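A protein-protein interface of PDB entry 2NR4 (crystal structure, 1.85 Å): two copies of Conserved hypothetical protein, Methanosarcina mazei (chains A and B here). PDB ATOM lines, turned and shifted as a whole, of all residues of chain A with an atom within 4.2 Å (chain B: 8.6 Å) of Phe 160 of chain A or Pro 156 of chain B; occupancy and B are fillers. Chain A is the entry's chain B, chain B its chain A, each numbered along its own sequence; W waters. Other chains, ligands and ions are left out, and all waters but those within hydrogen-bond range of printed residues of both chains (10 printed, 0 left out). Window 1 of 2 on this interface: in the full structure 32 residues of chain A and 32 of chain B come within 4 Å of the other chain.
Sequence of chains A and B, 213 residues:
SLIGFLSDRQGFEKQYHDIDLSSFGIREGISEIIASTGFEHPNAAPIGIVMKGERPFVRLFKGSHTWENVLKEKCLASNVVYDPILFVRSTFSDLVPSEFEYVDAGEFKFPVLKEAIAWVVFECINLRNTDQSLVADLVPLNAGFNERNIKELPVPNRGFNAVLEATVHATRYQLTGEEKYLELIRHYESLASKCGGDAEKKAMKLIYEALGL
The backbone carbonyl oxygen of Ile 30 of chain B lies within hydrogen-bond range of the side-chain amide nitrogen of Asn 157 of chain A (3.2 Å).
The backbone carbonyl oxygen of Pro 154 of chain B is in hydrogen-bond range of the side-chain hydroxyl of Tyr 82 of chain A (2.6 Å).
The backbone carbonyl oxygen (O) of Pro 156 of chain B is in hydrogen-bond range of the backbone NH (N) of Glu 32 of chain A (2.8 Å).
ND2 of Asn 157 of chain B sits at hydrogen-bond distance from O of Ile 30 of chain A, 3.2 Å away.
The side-chain amide oxygen (OD1) of Asn 161 of chain B sits at hydrogen-bond distance from the side-chain amide nitrogen (ND2) of Asn 161 of chain A, 3.2 Å away.
The side-chain carboxylate (OE2) of Glu 165 of chain B is in salt-bridge range of the guanidinium group (NE) of Arg 158 of chain A (2.7 Å).
O of Cys 195 of chain B sits at hydrogen-bond distance from N of Ile 30 of chain A (2.8 Å).
N of Gly 159 of chain B lies within hydrogen-bond range of OD1 of Asn 157 of chain B, at 2.8 Å.
N of Phe 160 of chain B sits at hydrogen-bond distance from OD1 of Asn 157 of chain B (2.9 Å).
The backbone carbonyl oxygen (O) of Asn 157 of chain B lies close to the side-chain amide oxygen (OD1) of Asn 161 of chain B, 3.2 Å away.
O of Cys 195 of chain B sits at hydrogen-bond distance from ND2 of Asn 157 of chain B, at 3.2 Å.
OD1 of Asn 157 of chain A lies within hydrogen-bond range of N of Gly 159 of chain A (2.9 Å).
The backbone carbonyl oxygen of Asn 157 of chain A sits close to the side-chain amide oxygen of Asn 161 of chain A (3.2 Å).
Among the printed residues, pairs that only touch across the chains: Ile 30 of chain A with Pro 156 of chain B (3.98 Å), Ser 31 of chain A with Val 155 of chain B (3.8 Å), Ser 31 of chain A with Pro 156 of chain B (3.7 Å), Glu 32 of chain A with Val 155 of chain B (3.9 Å), Glu 32 of chain A with Arg 158 of chain B (3.4 Å), Tyr 82 of chain A with Leu 153 of chain B (3.7 Å), Asn 157 of chain A with Glu 28 of chain B (3.9 Å), Phe 160 of chain A with Pro 156 of chain B (3.8 Å), Leu 164 of chain A with Arg 158 of chain B (3.8 Å) and Leu 164 of chain A with Asn 161 of chain B (3.7 Å).
Phe 160 of chain A touches one residue of chain B.
Of the printed residues of chain A, Pro 156 of chain B touches Ile 30, Ser 31, Glu 32 and Phe 160.
No residue of chain B comes within 4 Å of Gly 159 of chain A.
Of the printed residues of chain A, Leu 153 of chain B touches Tyr 82.
Printed residues of chain A within 4 Å of Ile 30 of chain B: Asn 157 (3.2 Å).
Of the printed residues of chain A, Glu 28 of chain B touches Asn 157.
Of the printed residues of chain A, Cys 195 of chain B touches Ile 30 (2.8 Å).
Arg 27 of chain B touches none of the printed residues of chain A.
Gly 29 of chain B touches none of the printed residues of chain A.
The nearest printed residue of chain B that does not touch Arg 158 of chain A is Ile 30 of chain B (4.6 Å).
Of the 15 printed residues of chain A, 9 touch a printed residue of chain B.
Hydrophobic or aromatic side chains of chain A that line the printed part of chain B: Ile 30, Tyr 82, Phe 160 and Leu 164.
Among the printed residues, 17 pairs touch across the chains.
Among the printed residues, Asp or Glu carboxylates within 4 Å of a Lys or Arg side-chain nitrogen of the other chain: Arg 158 of chain A with Glu 165 of chain B (2.7 Å).
Ile 30 of chain A touches Asn 157 of chain B, and with the chains exchanged Asn 157 of chain A touches Ile 30 of chain B.
Asn 161 of chain B touches its own counterpart, Asn 161 of chain A.
6 positions are printed for both chains.
Of the 17 pairs that touch across the chains among the printed residues, 3 have their exchanged pair printed and touching as well.
Water W2 lies within hydrogen-bond range of the side-chain carboxylate of Glu 32 of chain A (2.6 Å), the backbone carbonyl oxygen of Ile 30 of chain A (2.7 Å), the backbone NH of Arg 158 of chain B (2.8 Å) and the side-chain sulfur of Cys 195 of chain B (3.8 Å).
Water W1 bridges O of Ile 30 of chain B (2.7 Å) and N of Arg 158 of chain A (2.8 Å).
Water W3 bridges ND2 of Asn 157 of chain B (2.8 Å) and OG of Ser 31 of chain A (2.9 Å).
Water W10 bridges the side-chain amide nitrogen of Asn 161 of chain B and the backbone carbonyl oxygen of Asn 161 of chain A.
Water W4 lies within hydrogen-bond range of the side-chain carboxylate of Glu 165 of chain B (2.9 Å) and the backbone carbonyl oxygen of Arg 158 of chain A (2.9 Å).
Water W6 lies within hydrogen-bond range of the side-chain amide oxygen of Asn 161 of chain A and the side-chain amide nitrogen of Asn 161 of chain B.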
ATOM      1  N   ILE A  30      -0.703  12.872 -20.074  1.00  0.00           N
ATOM      2  CA  ILE A  30       0.188  13.458 -21.105  1.00  0.00           C
ATOM      3  C   ILE A  30       0.183  14.986 -20.982  1.00  0.00           C
ATOM      4  O   ILE A  30      -0.852  15.609 -21.222  1.00  0.00           O
ATOM      5  CB  ILE A  30      -0.161  12.981 -22.500  1.00  0.00           C
ATOM      6  CG1 ILE A  30      -0.111  11.429 -22.564  1.00  0.00           C
ATOM      7  CG2 ILE A  30       0.767  13.655 -23.558  1.00  0.00           C
ATOM      8  CD1 ILE A  30      -0.419  10.839 -23.934  1.00  0.00           C
ATOM      9  N   SER A  31       1.333  15.577 -20.601  1.00  0.00           N
ATOM     10  CA  SER A  31       1.433  17.023 -20.400  1.00  0.00           C
ATOM     11  C   SER A  31       1.927  17.615 -21.725  1.00  0.00           C
ATOM     12  O   SER A  31       2.977  17.197 -22.228  1.00  0.00           O
ATOM     13  CB  SER A  31       2.443  17.343 -19.296  1.00  0.00           C
ATOM     14  OG  SER A  31       2.162  16.594 -18.119  1.00  0.00           O
ATOM     15  N   GLU A  32       1.159  18.536 -22.315  1.00  0.00           N
ATOM     16  CA  GLU A  32       1.492  19.066 -23.638  1.00  0.00           C
ATOM     17  C   GLU A  32       2.416  20.288 -23.430  1.00  0.00           C
ATOM     18  O   GLU A  32       1.979  21.354 -22.959  1.00  0.00           O
ATOM     19  CB  GLU A  32       0.247  19.413 -24.466  1.00  0.00           C
ATOM     20  CG  GLU A  32      -0.774  18.213 -24.581  1.00  0.00           C
ATOM     21  CD  GLU A  32      -0.284  17.082 -25.466  1.00  0.00           C
ATOM     22  OE1 GLU A  32       0.689  17.274 -26.248  1.00  0.00           O
ATOM     23  OE2 GLU A  32      -0.910  15.991 -25.433  1.00  0.00           O
ATOM     24  N   VAL A  81       4.381  26.176 -21.630  1.00  0.00           N
ATOM     25  CA  VAL A  81       4.003  27.393 -22.351  1.00  0.00           C
ATOM     26  C   VAL A  81       2.448  27.529 -22.357  1.00  0.00           C
ATOM     27  O   VAL A  81       1.744  26.582 -22.675  1.00  0.00           O
ATOM     28  CB  VAL A  81       4.576  27.254 -23.783  1.00  0.00           C
ATOM     29  CG1 VAL A  81       3.859  28.119 -24.788  1.00  0.00           C
ATOM     30  CG2 VAL A  81       6.118  27.553 -23.736  1.00  0.00           C
ATOM     31  N   TYR A  82       1.927  28.694 -22.006  1.00  0.00           N
ATOM     32  CA  TYR A  82       0.479  28.884 -22.091  1.00  0.00           C
ATOM     33  C   TYR A  82       0.092  29.750 -23.300  1.00  0.00           C
ATOM     34  O   TYR A  82      -1.079  30.010 -23.538  1.00  0.00           O
ATOM     35  CB  TYR A  82      -0.024  29.585 -20.831  1.00  0.00           C
ATOM     36  CG  TYR A  82       0.282  28.868 -19.535  1.00  0.00           C
ATOM     37  CD1 TYR A  82       0.083  27.492 -19.403  1.00  0.00           C
ATOM     38  CD2 TYR A  82       0.705  29.583 -18.414  1.00  0.00           C
ATOM     39  CE1 TYR A  82       0.367  26.840 -18.193  1.00  0.00           C
ATOM     40  CE2 TYR A  82       0.950  28.939 -17.199  1.00  0.00           C
ATOM     41  CZ  TYR A  82       0.774  27.573 -17.097  1.00  0.00           C
ATOM     42  OH  TYR A  82       1.017  26.910 -15.900  1.00  0.00           O
ATOM     43  N   PRO A  84      -0.536  30.486 -27.069  1.00  0.00           N
ATOM     44  CA  PRO A  84      -0.875  29.640 -28.226  1.00  0.00           C
ATOM     45  C   PRO A  84      -0.009  30.019 -29.439  1.00  0.00           C
ATOM     46  O   PRO A  84       0.255  29.177 -30.299  1.00  0.00           O
ATOM     47  CB  PRO A  84      -2.364  29.968 -28.486  1.00  0.00           C
ATOM     48  CG  PRO A  84      -2.553  31.329 -27.893  1.00  0.00           C
ATOM     49  CD  PRO A  84      -1.600  31.455 -26.741  1.00  0.00           C
ATOM     50  N   ASN A 157      -9.917  27.432 -21.556  1.00  0.00           N
ATOM     51  CA  ASN A 157     -10.400  28.255 -22.666  1.00  0.00           C
ATOM     52  C   ASN A 157     -10.504  27.311 -23.829  1.00  0.00           C
ATOM     53  O   ASN A 157      -9.496  26.719 -24.231  1.00  0.00           O
ATOM     54  CB  ASN A 157      -9.429  29.399 -22.989  1.00  0.00           C
ATOM     55  CG  ASN A 157      -9.895  30.265 -24.171  1.00  0.00           C
ATOM     56  OD1 ASN A 157      -9.815  29.851 -25.311  1.00  0.00           O
ATOM     57  ND2 ASN A 157     -10.316  31.511 -23.892  1.00  0.00           N
ATOM     58  N   ARG A 158     -11.707  27.135 -24.368  1.00  0.00           N
ATOM     59  CA  ARG A 158     -11.931  26.152 -25.424  1.00  0.00           C
ATOM     60  C   ARG A 158     -11.279  26.588 -26.747  1.00  0.00           C
ATOM     61  O   ARG A 158     -10.985  25.771 -27.593  1.00  0.00           O
ATOM     62  CB  ARG A 158     -13.426  25.934 -25.650  1.00  0.00           C
ATOM     63  CG  ARG A 158     -14.073  25.178 -24.518  1.00  0.00           C
ATOM     64  CD  ARG A 158     -15.577  25.100 -24.739  1.00  0.00           C
ATOM     65  NE  ARG A 158     -15.893  24.172 -25.804  1.00  0.00           N
ATOM     66  CZ  ARG A 158     -17.012  24.205 -26.512  1.00  0.00           C
ATOM     67  NH1 ARG A 158     -17.902  25.168 -26.294  1.00  0.00           N
ATOM     68  NH2 ARG A 158     -17.211  23.316 -27.466  1.00  0.00           N
ATOM     69  N   GLY A 159     -11.118  27.888 -26.920  1.00  0.00           N
ATOM     70  CA  GLY A 159     -10.408  28.453 -28.077  1.00  0.00           C
ATOM     71  C   GLY A 159      -8.920  28.099 -28.060  1.00  0.00           C
ATOM     72  O   GLY A 159      -8.380  27.691 -29.098  1.00  0.00           O
ATOM     73  N   PHE A 160      -8.258  28.249 -26.907  1.00  0.00           N
ATOM     74  CA  PHE A 160      -6.864  27.753 -26.757  1.00  0.00           C
ATOM     75  C   PHE A 160      -6.829  26.217 -26.974  1.00  0.00           C
ATOM     76  O   PHE A 160      -5.949  25.673 -27.691  1.00  0.00           O
ATOM     77  CB  PHE A 160      -6.316  28.095 -25.375  1.00  0.00           C
ATOM     78  CG  PHE A 160      -4.931  27.533 -25.137  1.00  0.00           C
ATOM     79  CD1 PHE A 160      -3.794  28.295 -25.454  1.00  0.00           C
ATOM     80  CD2 PHE A 160      -4.758  26.219 -24.660  1.00  0.00           C
ATOM     81  CE1 PHE A 160      -2.502  27.757 -25.252  1.00  0.00           C
ATOM     82  CE2 PHE A 160      -3.470  25.676 -24.447  1.00  0.00           C
ATOM     83  CZ  PHE A 160      -2.339  26.441 -24.766  1.00  0.00           C
ATOM     84  N   ASN A 161      -7.801  25.503 -26.386  1.00  0.00           N
ATOM     85  CA  ASN A 161      -7.834  24.061 -26.602  1.00  0.00           C
ATOM     86  C   ASN A 161      -7.962  23.687 -28.069  1.00  0.00           C
ATOM     87  O   ASN A 161      -7.390  22.657 -28.527  1.00  0.00           O
ATOM     88  CB  ASN A 161      -8.913  23.395 -25.742  1.00  0.00           C
ATOM     89  CG  ASN A 161      -8.715  23.663 -24.280  1.00  0.00           C
ATOM     90  OD1 ASN A 161      -7.647  24.194 -23.845  1.00  0.00           O
ATOM     91  ND2 ASN A 161      -9.749  23.316 -23.477  1.00  0.00           N
ATOM     92  N   ALA A 162      -8.752  24.486 -28.799  1.00  0.00           N
ATOM     93  CA  ALA A 162      -8.939  24.293 -30.247  1.00  0.00           C
ATOM     94  C   ALA A 162      -7.645  24.526 -31.058  1.00  0.00           C
ATOM     95  O   ALA A 162      -7.367  23.792 -32.023  1.00  0.00           O
ATOM     96  CB  ALA A 162     -10.042  25.238 -30.755  1.00  0.00           C
ATOM     97  N   VAL A 163      -6.888  25.574 -30.710  1.00  0.00           N
ATOM     98  CA  VAL A 163      -5.564  25.813 -31.321  1.00  0.00           C
ATOM     99  C   VAL A 163      -4.686  24.586 -31.054  1.00  0.00           C
ATOM    100  O   VAL A 163      -4.013  24.077 -31.964  1.00  0.00           O
ATOM    101  CB  VAL A 163      -4.889  27.094 -30.776  1.00  0.00           C
ATOM    102  CG1 VAL A 163      -3.432  27.259 -31.361  1.00  0.00           C
ATOM    103  CG2 VAL A 163      -5.720  28.337 -31.157  1.00  0.00           C
ATOM    104  N   LEU A 164      -4.722  24.068 -29.822  1.00  0.00           N
ATOM    105  CA  LEU A 164      -3.880  22.905 -29.500  1.00  0.00           C
ATOM    106  C   LEU A 164      -4.265  21.719 -30.415  1.00  0.00           C
ATOM    107  O   LEU A 164      -3.396  21.043 -31.015  1.00  0.00           O
ATOM    108  CB  LEU A 164      -4.070  22.540 -28.015  1.00  0.00           C
ATOM    109  CG  LEU A 164      -3.259  21.368 -27.461  1.00  0.00           C
ATOM    110  CD1 LEU A 164      -1.752  21.626 -27.589  1.00  0.00           C
ATOM    111  CD2 LEU A 164      -3.598  21.142 -25.925  1.00  0.00           C
ATOM    112  N   GLU A 200      -5.241  33.608 -29.395  1.00  0.00           N
ATOM    113  CA  GLU A 200      -5.725  32.383 -30.003  1.00  0.00           C
ATOM    114  C   GLU A 200      -6.109  32.627 -31.438  1.00  0.00           C
ATOM    115  O   GLU A 200      -5.819  31.816 -32.317  1.00  0.00           O
ATOM    116  CB  GLU A 200      -6.902  31.768 -29.217  1.00  0.00           C
ATOM    117  CG  GLU A 200      -6.460  31.105 -27.887  1.00  0.00           C
ATOM    118  CD  GLU A 200      -6.171  32.095 -26.772  1.00  0.00           C
ATOM    119  OE1 GLU A 200      -6.724  33.229 -26.816  1.00  0.00           O
ATOM    120  OE2 GLU A 200      -5.398  31.746 -25.844  1.00  0.00           O
ATOM    121  N   ARG B  27     -10.086  36.158 -18.200  1.00  0.00           N
ATOM    122  CA  ARG B  27      -9.130  36.546 -19.247  1.00  0.00           C
ATOM    123  C   ARG B  27      -9.857  36.858 -20.524  1.00  0.00           C
ATOM    124  O   ARG B  27     -11.060  36.574 -20.673  1.00  0.00           O
ATOM    125  CB  ARG B  27      -8.181  35.397 -19.575  1.00  0.00           C
ATOM    126  CG  ARG B  27      -7.691  34.564 -18.434  1.00  0.00           C
ATOM    127  CD  ARG B  27      -6.458  35.102 -17.882  1.00  0.00           C
ATOM    128  NE  ARG B  27      -5.420  35.175 -18.918  1.00  0.00           N
ATOM    129  CZ  ARG B  27      -4.472  34.265 -19.109  1.00  0.00           C
ATOM    130  NH1 ARG B  27      -4.419  33.178 -18.338  1.00  0.00           N
ATOM    131  NH2 ARG B  27      -3.567  34.453 -20.077  1.00  0.00           N
ATOM    132  N   GLU B  28      -9.102  37.388 -21.502  1.00  0.00           N
ATOM    133  CA  GLU B  28      -9.673  37.671 -22.791  1.00  0.00           C
ATOM    134  C   GLU B  28     -10.285  36.405 -23.426  1.00  0.00           C
ATOM    135  O   GLU B  28      -9.723  35.324 -23.284  1.00  0.00           O
ATOM    136  CB  GLU B  28      -8.590  38.262 -23.701  1.00  0.00           C
ATOM    137  CG  GLU B  28      -9.165  38.936 -24.924  1.00  0.00           C
ATOM    138  CD  GLU B  28      -8.087  39.180 -26.004  1.00  0.00           C
ATOM    139  OE1 GLU B  28      -6.870  39.038 -25.718  1.00  0.00           O
ATOM    140  OE2 GLU B  28      -8.482  39.500 -27.136  1.00  0.00           O
ATOM    141  N   GLY B  29     -11.413  36.551 -24.124  1.00  0.00           N
ATOM    142  CA  GLY B  29     -12.103  35.409 -24.763  1.00  0.00           C
ATOM    143  C   GLY B  29     -13.126  34.852 -23.790  1.00  0.00           C
ATOM    144  O   GLY B  29     -13.648  35.608 -22.962  1.00  0.00           O
ATOM    145  N   ILE B  30     -13.410  33.548 -23.850  1.00  0.00           N
ATOM    146  CA  ILE B  30     -14.474  32.986 -22.991  1.00  0.00           C
ATOM    147  C   ILE B  30     -13.763  32.073 -22.023  1.00  0.00           C
ATOM    148  O   ILE B  30     -13.170  31.058 -22.443  1.00  0.00           O
ATOM    149  CB  ILE B  30     -15.559  32.263 -23.803  1.00  0.00           C
ATOM    150  CG1 ILE B  30     -16.250  33.241 -24.780  1.00  0.00           C
ATOM    151  CG2 ILE B  30     -16.643  31.691 -22.855  1.00  0.00           C
ATOM    152  CD1 ILE B  30     -17.270  32.549 -25.665  1.00  0.00           C
ATOM    153  N   LEU B 153       1.677  22.683 -10.981  1.00  0.00           N
ATOM    154  CA  LEU B 153       1.646  23.701 -12.042  1.00  0.00           C
ATOM    155  C   LEU B 153       0.617  23.289 -13.085  1.00  0.00           C
ATOM    156  O   LEU B 153       0.710  22.192 -13.581  1.00  0.00           O
ATOM    157  CB  LEU B 153       3.021  23.770 -12.759  1.00  0.00           C
ATOM    158  CG  LEU B 153       3.212  25.010 -13.636  1.00  0.00           C
ATOM    159  CD1 LEU B 153       3.107  26.257 -12.811  1.00  0.00           C
ATOM    160  CD2 LEU B 153       4.564  24.986 -14.423  1.00  0.00           C
ATOM    161  N   PRO B 154      -0.332  24.172 -13.461  1.00  0.00           N
ATOM    162  CA  PRO B 154      -1.242  23.843 -14.560  1.00  0.00           C
ATOM    163  C   PRO B 154      -0.460  23.628 -15.852  1.00  0.00           C
ATOM    164  O   PRO B 154       0.531  24.331 -16.079  1.00  0.00           O
ATOM    165  CB  PRO B 154      -2.076  25.128 -14.705  1.00  0.00           C
ATOM    166  CG  PRO B 154      -2.003  25.756 -13.369  1.00  0.00           C
ATOM    167  CD  PRO B 154      -0.637  25.510 -12.902  1.00  0.00           C
ATOM    168  N   VAL B 155      -0.890  22.674 -16.664  1.00  0.00           N
ATOM    169  CA  VAL B 155      -0.228  22.419 -17.960  1.00  0.00           C
ATOM    170  C   VAL B 155      -1.305  21.974 -18.936  1.00  0.00           C
ATOM    171  O   VAL B 155      -2.250  21.254 -18.497  1.00  0.00           O
ATOM    172  CB  VAL B 155       0.912  21.361 -17.828  1.00  0.00           C
ATOM    173  CG1 VAL B 155       0.334  19.953 -17.574  1.00  0.00           C
ATOM    174  CG2 VAL B 155       1.788  21.313 -19.108  1.00  0.00           C
ATOM    175  N   PRO B 156      -1.191  22.353 -20.242  1.00  0.00           N
ATOM    176  CA  PRO B 156      -2.194  21.840 -21.192  1.00  0.00           C
ATOM    177  C   PRO B 156      -2.256  20.300 -21.207  1.00  0.00           C
ATOM    178  O   PRO B 156      -1.209  19.573 -21.201  1.00  0.00           O
ATOM    179  CB  PRO B 156      -1.726  22.426 -22.543  1.00  0.00           C
ATOM    180  CG  PRO B 156      -1.100  23.789 -22.118  1.00  0.00           C
ATOM    181  CD  PRO B 156      -0.262  23.288 -20.926  1.00  0.00           C
ATOM    182  N   ASN B 157      -3.489  19.802 -21.146  1.00  0.00           N
ATOM    183  CA  ASN B 157      -3.721  18.363 -21.140  1.00  0.00           C
ATOM    184  C   ASN B 157      -4.960  18.094 -21.998  1.00  0.00           C
ATOM    185  O   ASN B 157      -6.075  18.581 -21.690  1.00  0.00           O
ATOM    186  CB  ASN B 157      -3.869  17.890 -19.693  1.00  0.00           C
ATOM    187  CG  ASN B 157      -4.090  16.388 -19.591  1.00  0.00           C
ATOM    188  OD1 ASN B 157      -5.112  15.860 -20.046  1.00  0.00           O
ATOM    189  ND2 ASN B 157      -3.140  15.695 -18.991  1.00  0.00           N
ATOM    190  N   ARG B 158      -4.762  17.356 -23.088  1.00  0.00           N
ATOM    191  CA  ARG B 158      -5.829  17.105 -24.033  1.00  0.00           C
ATOM    192  C   ARG B 158      -6.928  16.216 -23.430  1.00  0.00           C
ATOM    193  O   ARG B 158      -8.025  16.215 -23.949  1.00  0.00           O
ATOM    194  CB  ARG B 158      -5.290  16.455 -25.295  1.00  0.00           C
ATOM    195  CG  ARG B 158      -4.338  17.383 -26.112  1.00  0.00           C
ATOM    196  CD  ARG B 158      -3.728  16.540 -27.190  1.00  0.00           C
ATOM    197  NE  ARG B 158      -4.672  16.314 -28.262  1.00  0.00           N
ATOM    198  CZ  ARG B 158      -4.642  15.246 -29.052  1.00  0.00           C
ATOM    199  NH1 ARG B 158      -3.710  14.298 -28.877  1.00  0.00           N
ATOM    200  NH2 ARG B 158      -5.523  15.140 -30.017  1.00  0.00           N
ATOM    201  N   GLY B 159      -6.590  15.450 -22.393  1.00  0.00           N
ATOM    202  CA  GLY B 159      -7.554  14.610 -21.655  1.00  0.00           C
ATOM    203  C   GLY B 159      -8.522  15.472 -20.864  1.00  0.00           C
ATOM    204  O   GLY B 159      -9.758  15.280 -20.931  1.00  0.00           O
ATOM    205  N   PHE B 160      -7.982  16.445 -20.136  1.00  0.00           N
ATOM    206  CA  PHE B 160      -8.829  17.420 -19.441  1.00  0.00           C
ATOM    207  C   PHE B 160      -9.698  18.173 -20.445  1.00  0.00           C
ATOM    208  O   PHE B 160     -10.913  18.311 -20.274  1.00  0.00           O
ATOM    209  CB  PHE B 160      -7.983  18.401 -18.627  1.00  0.00           C
ATOM    210  CG  PHE B 160      -8.810  19.452 -17.941  1.00  0.00           C
ATOM    211  CD1 PHE B 160      -9.344  19.194 -16.679  1.00  0.00           C
ATOM    212  CD2 PHE B 160      -9.137  20.668 -18.586  1.00  0.00           C
ATOM    213  CE1 PHE B 160     -10.152  20.120 -16.034  1.00  0.00           C
ATOM    214  CE2 PHE B 160      -9.963  21.629 -17.935  1.00  0.00           C
ATOM    215  CZ  PHE B 160     -10.482  21.341 -16.640  1.00  0.00           C
ATOM    216  N   ASN B 161      -9.075  18.616 -21.545  1.00  0.00           N
ATOM    217  CA  ASN B 161      -9.810  19.341 -22.572  1.00  0.00           C
ATOM    218  C   ASN B 161     -10.927  18.489 -23.175  1.00  0.00           C
ATOM    219  O   ASN B 161     -11.998  18.995 -23.499  1.00  0.00           O
ATOM    220  CB  ASN B 161      -8.834  19.804 -23.662  1.00  0.00           C
ATOM    221  CG  ASN B 161      -7.785  20.766 -23.140  1.00  0.00           C
ATOM    222  OD1 ASN B 161      -7.830  21.246 -22.000  1.00  0.00           O
ATOM    223  ND2 ASN B 161      -6.790  21.054 -23.993  1.00  0.00           N
ATOM    224  N   GLU B 165     -15.083  19.166 -23.485  1.00  0.00           N
ATOM    225  CA  GLU B 165     -15.859  19.002 -24.701  1.00  0.00           C
ATOM    226  C   GLU B 165     -16.953  17.973 -24.499  1.00  0.00           C
ATOM    227  O   GLU B 165     -18.120  18.233 -24.877  1.00  0.00           O
ATOM    228  CB  GLU B 165     -14.957  18.611 -25.898  1.00  0.00           C
ATOM    229  CG  GLU B 165     -13.959  19.709 -26.282  1.00  0.00           C
ATOM    230  CD  GLU B 165     -14.617  21.038 -26.645  1.00  0.00           C
ATOM    231  OE1 GLU B 165     -15.597  21.030 -27.405  1.00  0.00           O
ATOM    232  OE2 GLU B 165     -14.188  22.093 -26.133  1.00  0.00           O
ATOM    233  N   CYS B 195      -4.793  10.514 -22.713  1.00  0.00           N
ATOM    234  CA  CYS B 195      -4.061  11.726 -22.254  1.00  0.00           C
ATOM    235  C   CYS B 195      -4.336  12.131 -20.821  1.00  0.00           C
ATOM    236  O   CYS B 195      -3.517  12.799 -20.184  1.00  0.00           O
ATOM    237  CB  CYS B 195      -4.335  12.932 -23.203  1.00  0.00           C
ATOM    238  SG  CYS B 195      -3.979  12.620 -24.964  1.00  0.00           S
HETATM  239  O   HOH W   1     -13.891  28.886 -23.835  1.00  0.00           O
HETATM  240  O   HOH W   2      -2.486  15.735 -23.429  1.00  0.00           O
HETATM  241  O   HOH W   3      -0.696  16.256 -17.649  1.00  0.00           O
HETATM  242  O   HOH W   4     -11.895  22.979 -27.604  1.00  0.00           O
HETATM  243  O   HOH W   5      -8.616  23.500 -20.598  1.00  0.00           O
HETATM  244  O   HOH W   6      -5.123  23.332 -22.725  1.00  0.00           O
HETATM  245  O   HOH W   7      -1.233  14.051 -27.219  1.00  0.00           O
HETATM  246  O   HOH W   8     -10.369  33.115 -21.383  1.00  0.00           O
HETATM  247  O   HOH W   9     -11.885  21.776 -24.453  1.00  0.00           O
HETATM  248  O   HOH W  10      -6.952  20.371 -26.756  1.00  0.00           O
